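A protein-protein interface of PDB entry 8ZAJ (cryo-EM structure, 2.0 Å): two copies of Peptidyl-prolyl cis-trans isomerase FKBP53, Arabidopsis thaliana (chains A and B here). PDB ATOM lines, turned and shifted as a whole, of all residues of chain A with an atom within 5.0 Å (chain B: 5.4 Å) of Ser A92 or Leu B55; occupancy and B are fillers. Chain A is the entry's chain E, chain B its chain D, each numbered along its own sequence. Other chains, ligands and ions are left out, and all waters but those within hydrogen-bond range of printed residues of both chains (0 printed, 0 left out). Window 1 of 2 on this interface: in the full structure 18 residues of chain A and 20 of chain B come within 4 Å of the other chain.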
ATOM      1  N   PHE A   3      24.210  16.561  -8.391  1.00  0.00           N
ATOM      2  CA  PHE A   3      23.398  16.980  -9.523  1.00  0.00           C
ATOM      3  C   PHE A   3      24.187  17.893 -10.454  1.00  0.00           C
ATOM      4  O   PHE A   3      25.006  18.703 -10.013  1.00  0.00           O
ATOM      5  CB  PHE A   3      22.138  17.694  -9.032  1.00  0.00           C
ATOM      6  CG  PHE A   3      21.331  18.316 -10.131  1.00  0.00           C
ATOM      7  CD1 PHE A   3      20.542  17.534 -10.953  1.00  0.00           C
ATOM      8  CD2 PHE A   3      21.358  19.684 -10.341  1.00  0.00           C
ATOM      9  CE1 PHE A   3      19.802  18.102 -11.966  1.00  0.00           C
ATOM     10  CE2 PHE A   3      20.616  20.257 -11.352  1.00  0.00           C
ATOM     11  CZ  PHE A   3      19.835  19.466 -12.164  1.00  0.00           C
ATOM     12  N   TRP A   4      23.938  17.747 -11.753  1.00  0.00           N
ATOM     13  CA  TRP A   4      24.558  18.574 -12.777  1.00  0.00           C
ATOM     14  C   TRP A   4      23.482  19.096 -13.717  1.00  0.00           C
ATOM     15  O   TRP A   4      22.525  18.383 -14.035  1.00  0.00           O
ATOM     16  CB  TRP A   4      25.615  17.790 -13.566  1.00  0.00           C
ATOM     17  CG  TRP A   4      26.216  18.559 -14.707  1.00  0.00           C
ATOM     18  CD1 TRP A   4      27.347  19.319 -14.676  1.00  0.00           C
ATOM     19  CD2 TRP A   4      25.716  18.639 -16.047  1.00  0.00           C
ATOM     20  NE1 TRP A   4      27.583  19.869 -15.911  1.00  0.00           N
ATOM     21  CE2 TRP A   4      26.595  19.467 -16.771  1.00  0.00           C
ATOM     22  CE3 TRP A   4      24.612  18.091 -16.705  1.00  0.00           C
ATOM     23  CZ2 TRP A   4      26.405  19.758 -18.118  1.00  0.00           C
ATOM     24  CZ3 TRP A   4      24.424  18.384 -18.041  1.00  0.00           C
ATOM     25  CH2 TRP A   4      25.315  19.209 -18.734  1.00  0.00           C
ATOM     26  N   GLY A   5      23.641  20.333 -14.156  1.00  0.00           N
ATOM     27  CA  GLY A   5      22.680  20.940 -15.059  1.00  0.00           C
ATOM     28  C   GLY A   5      23.338  21.999 -15.910  1.00  0.00           C
ATOM     29  O   GLY A   5      24.295  22.656 -15.487  1.00  0.00           O
ATOM     30  N   HIS A  26      27.605  13.101 -16.614  1.00  0.00           N
ATOM     31  CA  HIS A  26      26.662  12.156 -17.195  1.00  0.00           C
ATOM     32  C   HIS A  26      25.436  12.939 -17.643  1.00  0.00           C
ATOM     33  O   HIS A  26      24.649  13.396 -16.812  1.00  0.00           O
ATOM     34  CB  HIS A  26      26.275  11.071 -16.192  1.00  0.00           C
ATOM     35  CG  HIS A  26      27.325  10.024 -15.994  1.00  0.00           C
ATOM     36  ND1 HIS A  26      27.209   8.750 -16.504  1.00  0.00           N
ATOM     37  CD2 HIS A  26      28.507  10.060 -15.336  1.00  0.00           C
ATOM     38  CE1 HIS A  26      28.275   8.046 -16.171  1.00  0.00           C
ATOM     39  NE2 HIS A  26      29.079   8.817 -15.462  1.00  0.00           N
ATOM     40  N   VAL A  27      25.275  13.098 -18.953  1.00  0.00           N
ATOM     41  CA  VAL A  27      24.113  13.780 -19.508  1.00  0.00           C
ATOM     42  C   VAL A  27      23.037  12.717 -19.695  1.00  0.00           C
ATOM     43  O   VAL A  27      23.055  11.958 -20.663  1.00  0.00           O
ATOM     44  CB  VAL A  27      24.443  14.500 -20.814  1.00  0.00           C
ATOM     45  CG1 VAL A  27      23.218  15.228 -21.335  1.00  0.00           C
ATOM     46  CG2 VAL A  27      25.593  15.468 -20.606  1.00  0.00           C
ATOM     47  N   THR A  28      22.098  12.659 -18.755  1.00  0.00           N
ATOM     48  CA  THR A  28      21.077  11.625 -18.746  1.00  0.00           C
ATOM     49  C   THR A  28      19.709  12.120 -19.184  1.00  0.00           C
ATOM     50  O   THR A  28      18.774  11.318 -19.258  1.00  0.00           O
ATOM     51  CB  THR A  28      20.971  10.998 -17.352  1.00  0.00           C
ATOM     52  OG1 THR A  28      20.371  11.934 -16.447  1.00  0.00           O
ATOM     53  CG2 THR A  28      22.345  10.611 -16.840  1.00  0.00           C
ATOM     54  N   GLN A  29      19.564  13.406 -19.484  1.00  0.00           N
ATOM     55  CA  GLN A  29      18.270  13.925 -19.899  1.00  0.00           C
ATOM     56  C   GLN A  29      18.465  15.230 -20.649  1.00  0.00           C
ATOM     57  O   GLN A  29      19.333  16.033 -20.300  1.00  0.00           O
ATOM     58  CB  GLN A  29      17.345  14.140 -18.697  1.00  0.00           C
ATOM     59  CG  GLN A  29      15.887  14.338 -19.064  1.00  0.00           C
ATOM     60  CD  GLN A  29      15.125  13.033 -19.127  1.00  0.00           C
ATOM     61  OE1 GLN A  29      14.004  12.980 -19.634  1.00  0.00           O
ATOM     62  NE2 GLN A  29      15.728  11.970 -18.610  1.00  0.00           N
ATOM     63  N   THR A  31      15.850  18.306 -21.724  1.00  0.00           N
ATOM     64  CA  THR A  31      14.502  18.814 -21.522  1.00  0.00           C
ATOM     65  C   THR A  31      14.336  20.116 -22.287  1.00  0.00           C
ATOM     66  O   THR A  31      15.190  21.004 -22.203  1.00  0.00           O
ATOM     67  CB  THR A  31      14.208  19.031 -20.035  1.00  0.00           C
ATOM     68  OG1 THR A  31      14.722  17.929 -19.278  1.00  0.00           O
ATOM     69  CG2 THR A  31      12.711  19.147 -19.801  1.00  0.00           C
ATOM     70  N   HIS A  90      17.675  22.150 -21.728  1.00  0.00           N
ATOM     71  CA  HIS A  90      18.293  21.921 -20.430  1.00  0.00           C
ATOM     72  C   HIS A  90      18.859  20.509 -20.393  1.00  0.00           C
ATOM     73  O   HIS A  90      18.119  19.533 -20.552  1.00  0.00           O
ATOM     74  CB  HIS A  90      17.284  22.120 -19.300  1.00  0.00           C
ATOM     75  CG  HIS A  90      16.699  23.496 -19.241  1.00  0.00           C
ATOM     76  ND1 HIS A  90      15.851  23.988 -20.209  1.00  0.00           N
ATOM     77  CD2 HIS A  90      16.834  24.482 -18.322  1.00  0.00           C
ATOM     78  CE1 HIS A  90      15.492  25.218 -19.892  1.00  0.00           C
ATOM     79  NE2 HIS A  90      16.074  25.542 -18.752  1.00  0.00           N
ATOM     80  N   LEU A  91      20.163  20.401 -20.184  1.00  0.00           N
ATOM     81  CA  LEU A  91      20.814  19.116 -19.984  1.00  0.00           C
ATOM     82  C   LEU A  91      20.974  18.881 -18.491  1.00  0.00           C
ATOM     83  O   LEU A  91      21.516  19.733 -17.779  1.00  0.00           O
ATOM     84  CB  LEU A  91      22.175  19.070 -20.678  1.00  0.00           C
ATOM     85  CG  LEU A  91      22.204  19.410 -22.169  1.00  0.00           C
ATOM     86  CD1 LEU A  91      23.597  19.187 -22.731  1.00  0.00           C
ATOM     87  CD2 LEU A  91      21.179  18.587 -22.930  1.00  0.00           C
ATOM     88  N   SER A  92      20.500  17.736 -18.019  1.00  0.00           N
ATOM     89  CA  SER A  92      20.570  17.393 -16.611  1.00  0.00           C
ATOM     90  C   SER A  92      21.207  16.021 -16.445  1.00  0.00           C
ATOM     91  O   SER A  92      21.190  15.188 -17.353  1.00  0.00           O
ATOM     92  CB  SER A  92      19.180  17.417 -15.962  1.00  0.00           C
ATOM     93  OG  SER A  92      18.300  16.507 -16.597  1.00  0.00           O
ATOM     94  N   GLY A  93      21.779  15.803 -15.268  1.00  0.00           N
ATOM     95  CA  GLY A  93      22.436  14.537 -14.989  1.00  0.00           C
ATOM     96  C   GLY A  93      23.108  14.567 -13.638  1.00  0.00           C
ATOM     97  O   GLY A  93      22.572  15.120 -12.673  1.00  0.00           O
ATOM     98  N   PHE A  94      24.294  13.971 -13.583  1.00  0.00           N
ATOM     99  CA  PHE A  94      25.050  13.901 -12.344  1.00  0.00           C
ATOM    100  C   PHE A  94      26.536  13.847 -12.659  1.00  0.00           C
ATOM    101  O   PHE A  94      26.945  13.582 -13.790  1.00  0.00           O
ATOM    102  CB  PHE A  94      24.640  12.689 -11.492  1.00  0.00           C
ATOM    103  CG  PHE A  94      24.621  11.391 -12.246  1.00  0.00           C
ATOM    104  CD1 PHE A  94      23.492  10.993 -12.939  1.00  0.00           C
ATOM    105  CD2 PHE A  94      25.732  10.566 -12.255  1.00  0.00           C
ATOM    106  CE1 PHE A  94      23.472   9.799 -13.628  1.00  0.00           C
ATOM    107  CE2 PHE A  94      25.717   9.371 -12.943  1.00  0.00           C
ATOM    108  CZ  PHE A  94      24.585   8.987 -13.631  1.00  0.00           C
ATOM    109  N   VAL B  42       6.466  20.820 -15.549  1.00  0.00           N
ATOM    110  CA  VAL B  42       7.922  20.752 -15.501  1.00  0.00           C
ATOM    111  C   VAL B  42       8.366  20.804 -14.049  1.00  0.00           C
ATOM    112  O   VAL B  42       7.861  21.614 -13.264  1.00  0.00           O
ATOM    113  CB  VAL B  42       8.576  21.901 -16.298  1.00  0.00           C
ATOM    114  CG1 VAL B  42      10.087  21.747 -16.313  1.00  0.00           C
ATOM    115  CG2 VAL B  42       8.029  21.948 -17.703  1.00  0.00           C
ATOM    116  N   ILE B  43       9.312  19.942 -13.691  1.00  0.00           N
ATOM    117  CA  ILE B  43       9.958  19.976 -12.386  1.00  0.00           C
ATOM    118  C   ILE B  43      11.368  20.516 -12.574  1.00  0.00           C
ATOM    119  O   ILE B  43      12.142  19.989 -13.381  1.00  0.00           O
ATOM    120  CB  ILE B  43       9.967  18.591 -11.714  1.00  0.00           C
ATOM    121  CG1 ILE B  43      10.888  18.599 -10.491  1.00  0.00           C
ATOM    122  CG2 ILE B  43      10.367  17.507 -12.704  1.00  0.00           C
ATOM    123  CD1 ILE B  43      10.743  17.381  -9.607  1.00  0.00           C
ATOM    124  N   GLN B  44      11.696  21.574 -11.840  1.00  0.00           N
ATOM    125  CA  GLN B  44      12.985  22.240 -11.945  1.00  0.00           C
ATOM    126  C   GLN B  44      13.769  22.040 -10.659  1.00  0.00           C
ATOM    127  O   GLN B  44      13.211  22.121  -9.561  1.00  0.00           O
ATOM    128  CB  GLN B  44      12.813  23.734 -12.225  1.00  0.00           C
ATOM    129  CG  GLN B  44      12.548  24.062 -13.680  1.00  0.00           C
ATOM    130  CD  GLN B  44      12.141  25.505 -13.883  1.00  0.00           C
ATOM    131  OE1 GLN B  44      11.783  26.201 -12.932  1.00  0.00           O
ATOM    132  NE2 GLN B  44      12.191  25.965 -15.126  1.00  0.00           N
ATOM    133  N   CYS B  45      15.063  21.777 -10.799  1.00  0.00           N
ATOM    134  CA  CYS B  45      15.949  21.560  -9.665  1.00  0.00           C
ATOM    135  C   CYS B  45      16.914  22.733  -9.563  1.00  0.00           C
ATOM    136  O   CYS B  45      17.620  23.046 -10.528  1.00  0.00           O
ATOM    137  CB  CYS B  45      16.711  20.244  -9.810  1.00  0.00           C
ATOM    138  SG  CYS B  45      18.058  20.025  -8.628  1.00  0.00           S
ATOM    139  N   ILE B  53      17.349  24.185 -13.162  1.00  0.00           N
ATOM    140  CA  ILE B  53      17.554  23.367 -14.351  1.00  0.00           C
ATOM    141  C   ILE B  53      16.357  22.439 -14.495  1.00  0.00           C
ATOM    142  O   ILE B  53      16.031  21.693 -13.564  1.00  0.00           O
ATOM    143  CB  ILE B  53      18.865  22.562 -14.268  1.00  0.00           C
ATOM    144  CG1 ILE B  53      20.073  23.500 -14.297  1.00  0.00           C
ATOM    145  CG2 ILE B  53      18.943  21.546 -15.398  1.00  0.00           C
ATOM    146  CD1 ILE B  53      20.259  24.218 -15.613  1.00  0.00           C
ATOM    147  N   ALA B  54      15.707  22.486 -15.655  1.00  0.00           N
ATOM    148  CA  ALA B  54      14.522  21.671 -15.892  1.00  0.00           C
ATOM    149  C   ALA B  54      14.905  20.197 -15.954  1.00  0.00           C
ATOM    150  O   ALA B  54      15.658  19.779 -16.839  1.00  0.00           O
ATOM    151  CB  ALA B  54      13.833  22.103 -17.183  1.00  0.00           C
ATOM    152  N   LEU B  55      14.386  19.408 -15.009  1.00  0.00           N
ATOM    153  CA  LEU B  55      14.721  17.988 -14.964  1.00  0.00           C
ATOM    154  C   LEU B  55      14.002  17.210 -16.056  1.00  0.00           C
ATOM    155  O   LEU B  55      14.598  16.342 -16.702  1.00  0.00           O
ATOM    156  CB  LEU B  55      14.377  17.413 -13.592  1.00  0.00           C
ATOM    157  CG  LEU B  55      15.132  18.031 -12.420  1.00  0.00           C
ATOM    158  CD1 LEU B  55      14.863  17.261 -11.140  1.00  0.00           C
ATOM    159  CD2 LEU B  55      16.609  18.058 -12.736  1.00  0.00           C
ATOM    160  N   CYS B  56      12.724  17.504 -16.272  1.00  0.00           N
ATOM    161  CA  CYS B  56      11.927  16.782 -17.250  1.00  0.00           C
ATOM    162  C   CYS B  56      10.645  17.558 -17.495  1.00  0.00           C
ATOM    163  O   CYS B  56      10.252  18.413 -16.699  1.00  0.00           O
ATOM    164  CB  CYS B  56      11.611  15.360 -16.781  1.00  0.00           C
ATOM    165  SG  CYS B  56      10.297  15.264 -15.547  1.00  0.00           S
ATOM    166  N   SER B  57       9.997  17.246 -18.611  1.00  0.00           N
ATOM    167  CA  SER B  57       8.715  17.834 -18.965  1.00  0.00           C
ATOM    168  C   SER B  57       7.715  16.715 -19.204  1.00  0.00           C
ATOM    169  O   SER B  57       7.978  15.800 -19.990  1.00  0.00           O
ATOM    170  CB  SER B  57       8.835  18.723 -20.203  1.00  0.00           C
ATOM    171  OG  SER B  57       7.636  19.436 -20.434  1.00  0.00           O
ATOM    172  N   LEU B  68      14.163   8.774 -15.760  1.00  0.00           N
ATOM    173  CA  LEU B  68      15.191   9.721 -15.364  1.00  0.00           C
ATOM    174  C   LEU B  68      16.405   8.945 -14.886  1.00  0.00           C
ATOM    175  O   LEU B  68      16.321   7.761 -14.558  1.00  0.00           O
ATOM    176  CB  LEU B  68      14.708  10.672 -14.261  1.00  0.00           C
ATOM    177  CG  LEU B  68      13.457  11.507 -14.535  1.00  0.00           C
ATOM    178  CD1 LEU B  68      12.975  12.162 -13.253  1.00  0.00           C
ATOM    179  CD2 LEU B  68      13.728  12.550 -15.604  1.00  0.00           C
ATOM    180  N   LEU B  70      19.077  10.422 -12.294  1.00  0.00           N
ATOM    181  CA  LEU B  70      19.606  11.501 -11.476  1.00  0.00           C
ATOM    182  C   LEU B  70      20.075  10.937 -10.145  1.00  0.00           C
ATOM    183  O   LEU B  70      19.451  10.029  -9.592  1.00  0.00           O
ATOM    184  CB  LEU B  70      18.558  12.589 -11.238  1.00  0.00           C
ATOM    185  CG  LEU B  70      18.084  13.343 -12.479  1.00  0.00           C
ATOM    186  CD1 LEU B  70      16.954  14.293 -12.124  1.00  0.00           C
ATOM    187  CD2 LEU B  70      19.239  14.092 -13.118  1.00  0.00           C
ATOM    188  N   PHE B  72      21.247  12.183  -6.291  1.00  0.00           N
ATOM    189  CA  PHE B  72      21.302  13.236  -5.289  1.00  0.00           C
ATOM    190  C   PHE B  72      21.979  12.694  -4.041  1.00  0.00           C
ATOM    191  O   PHE B  72      21.618  11.619  -3.551  1.00  0.00           O
ATOM    192  CB  PHE B  72      19.903  13.755  -4.954  1.00  0.00           C
ATOM    193  CG  PHE B  72      19.291  14.588  -6.041  1.00  0.00           C
ATOM    194  CD1 PHE B  72      19.664  15.909  -6.211  1.00  0.00           C
ATOM    195  CD2 PHE B  72      18.341  14.050  -6.892  1.00  0.00           C
ATOM    196  CE1 PHE B  72      19.102  16.679  -7.208  1.00  0.00           C
ATOM    197  CE2 PHE B  72      17.775  14.815  -7.890  1.00  0.00           C
ATOM    198  CZ  PHE B  72      18.155  16.131  -8.049  1.00  0.00           C
ATOM    199  N   PHE B  81      13.157  21.863  -5.141  1.00  0.00           N
ATOM    200  CA  PHE B  81      12.386  21.385  -6.281  1.00  0.00           C
ATOM    201  C   PHE B  81      11.242  22.350  -6.559  1.00  0.00           C
ATOM    202  O   PHE B  81      10.475  22.690  -5.653  1.00  0.00           O
ATOM    203  CB  PHE B  81      11.842  19.979  -6.024  1.00  0.00           C
ATOM    204  CG  PHE B  81      12.883  18.901  -6.097  1.00  0.00           C
ATOM    205  CD1 PHE B  81      13.687  18.771  -7.213  1.00  0.00           C
ATOM    206  CD2 PHE B  81      13.049  18.011  -5.050  1.00  0.00           C
ATOM    207  CE1 PHE B  81      14.642  17.778  -7.283  1.00  0.00           C
ATOM    208  CE2 PHE B  81      14.003  17.016  -5.114  1.00  0.00           C
ATOM    209  CZ  PHE B  81      14.801  16.899  -6.232  1.00  0.00           C
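Hydrophobic or aromatic side chains of chain B that line the printed part of chain A: Ile B53, Ala B54, Leu B55, Leu B68, Leu B70 and Phe B72.
Printed residues of chain A that touch a printed residue of chain B: Phe A3, Gly A5, Gln A29, Thr A31, His A90, Leu A91, Ser A92 and Gly A93.
Among the printed residues, 15 pairs touch across the chains.
Among the printed residues, no Asp or Glu carboxylate lies within 4 Å of a Lys or Arg side-chain nitrogen of the other chain.
Trp A4 touches none of the printed residues of chain B.
Printed residues of chain B within 4 Å of Gly A5: Ile B53 (3.7 Å).
Thr A28 touches none of the printed residues of chain B.
Printed residues of chain B within 4 Å of Thr A31: Ala B54, Leu B55, Cys B56 and Ser B57.
Leu B55 touches just these residues of chain A: Phe A3, Gln A29, Thr A31 and Ser A92.
Of the printed residues of chain A, Leu B68 touches Gln A29 (3.7 Å).
The nearest printed residue of chain A that does not touch Leu B55 is His A90 (5.8 Å).
OG1 of Thr A31 is in hydrogen-bond range of O of Ala B54 (3.2 Å).
The backbone carbonyl oxygen (O) of Leu B55 lies within hydrogen-bond range of the side-chain hydroxyl (OG1) of Thr A31, at 3.0 Å.
No position is printed for both chains.
The backbone carbonyl oxygen of Gln A29 is in hydrogen-bond range of the backbone NH of Ser A92, at 3.1 Å.
O of Trp A4 sits at hydrogen-bond distance from N of Gly A93 (3.0 Å).
N of Ile B53 is in hydrogen-bond range of O of Cys B45.
The backbone carbonyl oxygen of Ile B43 is in hydrogen-bond range of the backbone NH of Leu B55.
The backbone NH (N) of His A90 lies within hydrogen-bond range of the backbone carbonyl oxygen (O) of Thr A31, 2.8 Å away.
The backbone NH (N) of Thr A28 is in hydrogen-bond range of the backbone carbonyl oxygen (O) of Ser A92, 3.0 Å away.
Among the printed residues, merely in contact across the chains: Phe A3 with Leu B55 (3.3 Å), Gln A29 with Leu B55 (3.4 Å), Thr A31 with Cys B56 (3.5 Å), Gly A93 with Leu B70 (3.5 Å), His A90 with Ala B54 (3.5 Å), Thr A31 with Ser B57 (3.5 Å), Gln A29 with Leu B68 (3.7 Å), Phe A3 with Phe B72 (3.7 Å), Ser A92 with Leu B55 (3.7 Å), Gly A5 with Ile B53 (3.7 Å), Phe A3 with Cys B45 (3.7 Å), Phe A3 with Ile B53 (3.9 Å) and Leu A91 with Ile B53 (3.9 Å).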
